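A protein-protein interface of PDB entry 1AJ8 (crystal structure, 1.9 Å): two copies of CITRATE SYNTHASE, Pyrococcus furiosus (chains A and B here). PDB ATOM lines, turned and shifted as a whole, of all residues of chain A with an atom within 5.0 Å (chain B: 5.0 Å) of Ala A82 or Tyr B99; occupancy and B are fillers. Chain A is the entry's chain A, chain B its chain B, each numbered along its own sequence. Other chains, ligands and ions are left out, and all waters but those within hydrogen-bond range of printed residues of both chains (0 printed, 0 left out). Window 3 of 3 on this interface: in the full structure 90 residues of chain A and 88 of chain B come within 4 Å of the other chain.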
ATOM      1  N   GLU A  78       9.494  -2.052  17.342  1.00  0.00           N
ATOM      2  CA  GLU A  78       9.502  -0.616  17.069  1.00  0.00           C
ATOM      3  C   GLU A  78      10.096   0.171  18.241  1.00  0.00           C
ATOM      4  O   GLU A  78      10.847   1.128  18.043  1.00  0.00           O
ATOM      5  CB  GLU A  78       8.080  -0.120  16.798  1.00  0.00           C
ATOM      6  CG  GLU A  78       7.486  -0.590  15.481  1.00  0.00           C
ATOM      7  CD  GLU A  78       6.143   0.059  15.190  1.00  0.00           C
ATOM      8  OE1 GLU A  78       5.186  -0.165  15.965  1.00  0.00           O
ATOM      9  OE2 GLU A  78       6.045   0.798  14.188  1.00  0.00           O
ATOM     10  N   ILE A  79       9.755  -0.223  19.464  1.00  0.00           N
ATOM     11  CA  ILE A  79      10.295   0.464  20.631  1.00  0.00           C
ATOM     12  C   ILE A  79      11.802   0.197  20.703  1.00  0.00           C
ATOM     13  O   ILE A  79      12.578   1.089  21.032  1.00  0.00           O
ATOM     14  CB  ILE A  79       9.597  -0.006  21.936  1.00  0.00           C
ATOM     15  CG1 ILE A  79       8.186   0.598  22.015  1.00  0.00           C
ATOM     16  CG2 ILE A  79      10.420   0.395  23.152  1.00  0.00           C
ATOM     17  CD1 ILE A  79       8.155   2.117  22.161  1.00  0.00           C
ATOM     18  N   MET A  80      12.212  -1.030  20.381  1.00  0.00           N
ATOM     19  CA  MET A  80      13.633  -1.381  20.388  1.00  0.00           C
ATOM     20  C   MET A  80      14.367  -0.488  19.390  1.00  0.00           C
ATOM     21  O   MET A  80      15.469  -0.007  19.659  1.00  0.00           O
ATOM     22  CB  MET A  80      13.823  -2.845  19.996  1.00  0.00           C
ATOM     23  CG  MET A  80      13.499  -3.823  21.106  1.00  0.00           C
ATOM     24  SD  MET A  80      13.638  -5.546  20.600  1.00  0.00           S
ATOM     25  CE  MET A  80      15.459  -5.744  20.692  1.00  0.00           C
ATOM     26  N   GLU A  81      13.746  -0.267  18.237  1.00  0.00           N
ATOM     27  CA  GLU A  81      14.342   0.573  17.208  1.00  0.00           C
ATOM     28  C   GLU A  81      14.388   2.040  17.624  1.00  0.00           C
ATOM     29  O   GLU A  81      15.107   2.832  17.025  1.00  0.00           O
ATOM     30  CB  GLU A  81      13.569   0.432  15.899  1.00  0.00           C
ATOM     31  CG  GLU A  81      14.044  -0.726  15.040  1.00  0.00           C
ATOM     32  CD  GLU A  81      13.015  -1.168  14.008  1.00  0.00           C
ATOM     33  OE1 GLU A  81      11.948  -0.526  13.897  1.00  0.00           O
ATOM     34  OE2 GLU A  81      13.275  -2.166  13.302  1.00  0.00           O
ATOM     35  N   ALA A  82      13.635   2.399  18.660  1.00  0.00           N
ATOM     36  CA  ALA A  82      13.605   3.784  19.133  1.00  0.00           C
ATOM     37  C   ALA A  82      14.567   4.045  20.293  1.00  0.00           C
ATOM     38  O   ALA A  82      14.753   5.193  20.696  1.00  0.00           O
ATOM     39  CB  ALA A  82      12.181   4.165  19.551  1.00  0.00           C
ATOM     40  N   LEU A  83      15.172   2.992  20.835  1.00  0.00           N
ATOM     41  CA  LEU A  83      16.101   3.147  21.950  1.00  0.00           C
ATOM     42  C   LEU A  83      17.428   3.745  21.491  1.00  0.00           C
ATOM     43  O   LEU A  83      17.847   3.535  20.351  1.00  0.00           O
ATOM     44  CB  LEU A  83      16.370   1.789  22.602  1.00  0.00           C
ATOM     45  CG  LEU A  83      15.177   1.057  23.208  1.00  0.00           C
ATOM     46  CD1 LEU A  83      15.631  -0.302  23.724  1.00  0.00           C
ATOM     47  CD2 LEU A  83      14.583   1.892  24.331  1.00  0.00           C
ATOM     48  N   PRO A  84      18.097   4.520  22.364  1.00  0.00           N
ATOM     49  CA  PRO A  84      19.382   5.102  21.955  1.00  0.00           C
ATOM     50  C   PRO A  84      20.300   3.943  21.581  1.00  0.00           C
ATOM     51  O   PRO A  84      20.489   3.019  22.372  1.00  0.00           O
ATOM     52  CB  PRO A  84      19.856   5.849  23.199  1.00  0.00           C
ATOM     53  CG  PRO A  84      18.609   6.099  23.993  1.00  0.00           C
ATOM     54  CD  PRO A  84      17.725   4.914  23.735  1.00  0.00           C
ATOM     55  N   THR A  95      14.023  -1.723  29.821  1.00  0.00           N
ATOM     56  CA  THR A  95      12.967  -0.948  29.187  1.00  0.00           C
ATOM     57  C   THR A  95      12.026  -1.798  28.335  1.00  0.00           C
ATOM     58  O   THR A  95      10.809  -1.620  28.391  1.00  0.00           O
ATOM     59  CB  THR A  95      13.556   0.166  28.313  1.00  0.00           C
ATOM     60  OG1 THR A  95      14.377   1.010  29.120  1.00  0.00           O
ATOM     61  CG2 THR A  95      12.444   1.007  27.689  1.00  0.00           C
ATOM     62  N   GLU B  75      12.252  13.212  22.757  1.00  0.00           N
ATOM     63  CA  GLU B  75      12.261  11.762  22.580  1.00  0.00           C
ATOM     64  C   GLU B  75      11.472  11.034  23.664  1.00  0.00           C
ATOM     65  O   GLU B  75      10.911   9.963  23.422  1.00  0.00           O
ATOM     66  CB  GLU B  75      13.701  11.243  22.552  1.00  0.00           C
ATOM     67  CG  GLU B  75      14.757  12.332  22.609  1.00  0.00           C
ATOM     68  CD  GLU B  75      15.990  11.891  23.368  1.00  0.00           C
ATOM     69  OE1 GLU B  75      16.286  10.675  23.363  1.00  0.00           O
ATOM     70  OE2 GLU B  75      16.665  12.757  23.970  1.00  0.00           O
ATOM     71  N   VAL B  76      11.431  11.609  24.861  1.00  0.00           N
ATOM     72  CA  VAL B  76      10.686  10.992  25.955  1.00  0.00           C
ATOM     73  C   VAL B  76       9.185  11.147  25.726  1.00  0.00           C
ATOM     74  O   VAL B  76       8.419  10.205  25.917  1.00  0.00           O
ATOM     75  CB  VAL B  76      11.055  11.618  27.310  1.00  0.00           C
ATOM     76  CG1 VAL B  76      10.114  11.101  28.394  1.00  0.00           C
ATOM     77  CG2 VAL B  76      12.502  11.273  27.656  1.00  0.00           C
ATOM     78  N   ILE B  79       8.018   8.681  23.324  1.00  0.00           N
ATOM     79  CA  ILE B  79       7.824   7.357  23.887  1.00  0.00           C
ATOM     80  C   ILE B  79       6.483   7.315  24.623  1.00  0.00           C
ATOM     81  O   ILE B  79       5.769   6.309  24.585  1.00  0.00           O
ATOM     82  CB  ILE B  79       8.952   7.003  24.878  1.00  0.00           C
ATOM     83  CG1 ILE B  79      10.283   6.886  24.132  1.00  0.00           C
ATOM     84  CG2 ILE B  79       8.623   5.706  25.593  1.00  0.00           C
ATOM     85  CD1 ILE B  79      10.309   5.773  23.100  1.00  0.00           C
ATOM     86  N   THR B  95       7.989   2.507  32.724  1.00  0.00           N
ATOM     87  CA  THR B  95       8.616   2.437  31.408  1.00  0.00           C
ATOM     88  C   THR B  95       9.324   3.738  31.051  1.00  0.00           C
ATOM     89  O   THR B  95      10.432   3.726  30.507  1.00  0.00           O
ATOM     90  CB  THR B  95       7.575   2.093  30.317  1.00  0.00           C
ATOM     91  OG1 THR B  95       7.057   0.781  30.564  1.00  0.00           O
ATOM     92  CG2 THR B  95       8.207   2.123  28.924  1.00  0.00           C
ATOM     93  N   ILE B  96       8.696   4.865  31.368  1.00  0.00           N
ATOM     94  CA  ILE B  96       9.293   6.154  31.059  1.00  0.00           C
ATOM     95  C   ILE B  96      10.559   6.410  31.865  1.00  0.00           C
ATOM     96  O   ILE B  96      11.543   6.921  31.335  1.00  0.00           O
ATOM     97  CB  ILE B  96       8.288   7.293  31.297  1.00  0.00           C
ATOM     98  CG1 ILE B  96       7.090   7.105  30.367  1.00  0.00           C
ATOM     99  CG2 ILE B  96       8.942   8.640  31.039  1.00  0.00           C
ATOM    100  CD1 ILE B  96       7.490   6.943  28.910  1.00  0.00           C
ATOM    101  N   ILE B  97      10.535   6.064  33.148  1.00  0.00           N
ATOM    102  CA  ILE B  97      11.731   6.272  33.950  1.00  0.00           C
ATOM    103  C   ILE B  97      12.876   5.394  33.425  1.00  0.00           C
ATOM    104  O   ILE B  97      14.009   5.822  33.360  1.00  0.00           O
ATOM    105  CB  ILE B  97      11.485   5.998  35.439  1.00  0.00           C
ATOM    106  CG1 ILE B  97      10.412   6.943  35.981  1.00  0.00           C
ATOM    107  CG2 ILE B  97      12.781   6.144  36.222  1.00  0.00           C
ATOM    108  CD1 ILE B  97       9.944   6.602  37.378  1.00  0.00           C
ATOM    109  N   SER B  98      12.522   4.178  33.012  1.00  0.00           N
ATOM    110  CA  SER B  98      13.511   3.258  32.460  1.00  0.00           C
ATOM    111  C   SER B  98      14.144   3.876  31.214  1.00  0.00           C
ATOM    112  O   SER B  98      15.355   3.818  31.020  1.00  0.00           O
ATOM    113  CB  SER B  98      12.849   1.941  32.087  1.00  0.00           C
ATOM    114  OG  SER B  98      13.828   0.959  31.816  1.00  0.00           O
ATOM    115  N   TYR B  99      13.307   4.476  30.375  1.00  0.00           N
ATOM    116  CA  TYR B  99      13.777   5.114  29.154  1.00  0.00           C
ATOM    117  C   TYR B  99      14.654   6.322  29.469  1.00  0.00           C
ATOM    118  O   TYR B  99      15.678   6.537  28.822  1.00  0.00           O
ATOM    119  CB  TYR B  99      12.582   5.533  28.294  1.00  0.00           C
ATOM    120  CG  TYR B  99      12.975   6.168  26.983  1.00  0.00           C
ATOM    121  CD1 TYR B  99      13.442   5.393  25.922  1.00  0.00           C
ATOM    122  CD2 TYR B  99      12.909   7.546  26.811  1.00  0.00           C
ATOM    123  CE1 TYR B  99      13.838   5.982  24.725  1.00  0.00           C
ATOM    124  CE2 TYR B  99      13.301   8.141  25.621  1.00  0.00           C
ATOM    125  CZ  TYR B  99      13.765   7.355  24.587  1.00  0.00           C
ATOM    126  OH  TYR B  99      14.169   7.954  23.418  1.00  0.00           O
ATOM    127  N   LEU B 100      14.253   7.117  30.461  1.00  0.00           N
ATOM    128  CA  LEU B 100      15.031   8.284  30.849  1.00  0.00           C
ATOM    129  C   LEU B 100      16.426   7.802  31.224  1.00  0.00           C
ATOM    130  O   LEU B 100      17.429   8.475  30.962  1.00  0.00           O
ATOM    131  CB  LEU B 100      14.406   8.973  32.059  1.00  0.00           C
ATOM    132  CG  LEU B 100      13.532  10.213  31.851  1.00  0.00           C
ATOM    133  CD1 LEU B 100      12.969  10.625  33.203  1.00  0.00           C
ATOM    134  CD2 LEU B 100      14.329  11.351  31.243  1.00  0.00           C
ATOM    135  N   GLY B 101      16.478   6.636  31.858  1.00  0.00           N
ATOM    136  CA  GLY B 101      17.752   6.074  32.256  1.00  0.00           C
ATOM    137  C   GLY B 101      18.557   5.742  31.019  1.00  0.00           C
ATOM    138  O   GLY B 101      19.758   5.993  30.966  1.00  0.00           O
ATOM    139  N   ASN B 102      17.887   5.184  30.017  1.00  0.00           N
ATOM    140  CA  ASN B 102      18.543   4.817  28.766  1.00  0.00           C
ATOM    141  C   ASN B 102      19.189   6.005  28.059  1.00  0.00           C
ATOM    142  O   ASN B 102      20.283   5.881  27.503  1.00  0.00           O
ATOM    143  CB  ASN B 102      17.542   4.182  27.809  1.00  0.00           C
ATOM    144  CG  ASN B 102      17.066   2.830  28.272  1.00  0.00           C
ATOM    145  OD1 ASN B 102      17.712   2.168  29.095  1.00  0.00           O
ATOM    146  ND2 ASN B 102      15.929   2.405  27.746  1.00  0.00           N
ATOM    147  N   ILE B 103      18.516   7.152  28.066  1.00  0.00           N
ATOM    148  CA  ILE B 103      19.052   8.331  27.396  1.00  0.00           C
ATOM    149  C   ILE B 103      20.028   9.125  28.255  1.00  0.00           C
ATOM    150  O   ILE B 103      20.676  10.046  27.766  1.00  0.00           O
ATOM    151  CB  ILE B 103      17.915   9.279  26.904  1.00  0.00           C
ATOM    152  CG1 ILE B 103      17.159   9.875  28.087  1.00  0.00           C
ATOM    153  CG2 ILE B 103      16.938   8.517  26.024  1.00  0.00           C
ATOM    154  CD1 ILE B 103      16.009  10.786  27.667  1.00  0.00           C
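Of the 8 printed residues of chain A, 4 touch a printed residue of chain B.
Hydrophobic or aromatic side chains of chain A that line the printed part of chain B: Leu A83 and Pro A84.
Of the 12 printed residues of chain B, 4 touch a printed residue of chain A.
Printed residues of chain B that touch a printed residue of chain A: Ser B98, Tyr B99, Asn B102 and Ile B103.
Among the printed residues, no Asp or Glu carboxylate lies within 4 Å of a Lys or Arg side-chain nitrogen of the other chain.
OG of Ser B98 is in hydrogen-bond range of OG1 of Thr A95, 2.8 Å away.
The side-chain amide nitrogen (ND2) of Asn B102 is in hydrogen-bond range of the side-chain hydroxyl (OG1) of Thr A95 (2.5 Å).
The side-chain carboxylate of Glu B75 lies close to the side-chain hydroxyl of Tyr B99, 3.4 Å away.
O of Ser B98 sits close to OD1 of Asn B102, at 3.5 Å.
Of chain B, only Tyr B99 comes within 4 Å of Ala A82.
Printed residues of chain A within 4 Å of Tyr B99: Ala A82 and Thr A95.
Of the printed residues of chain B, Thr A95 touches Ser B98, Tyr B99 and Asn B102.
Of the printed residues of chain A, Ile B103 touches Pro A84 (3.6 Å).
Glu A78 touches none of the printed residues of chain B.
The nearest residue of chain B that does not touch Ala A82 is Ile B79 (4.3 Å).
OH of Tyr B99 touches O of Ala A82 (3.9 Å).
Leu A83 touches Asn B102.
Pro A84 touches Asn B102 (CG to O, 3.9 Å).
CG of Pro A84 touches CG2 of Ile B103 (3.6 Å).
OG1 of Thr A95 touches N of Tyr B99, 3.8 Å away.
2 positions are printed for both chains.
Of the 7 pairs that touch across the chains among the printed residues, none has its exchanged pair printed and touching as well.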
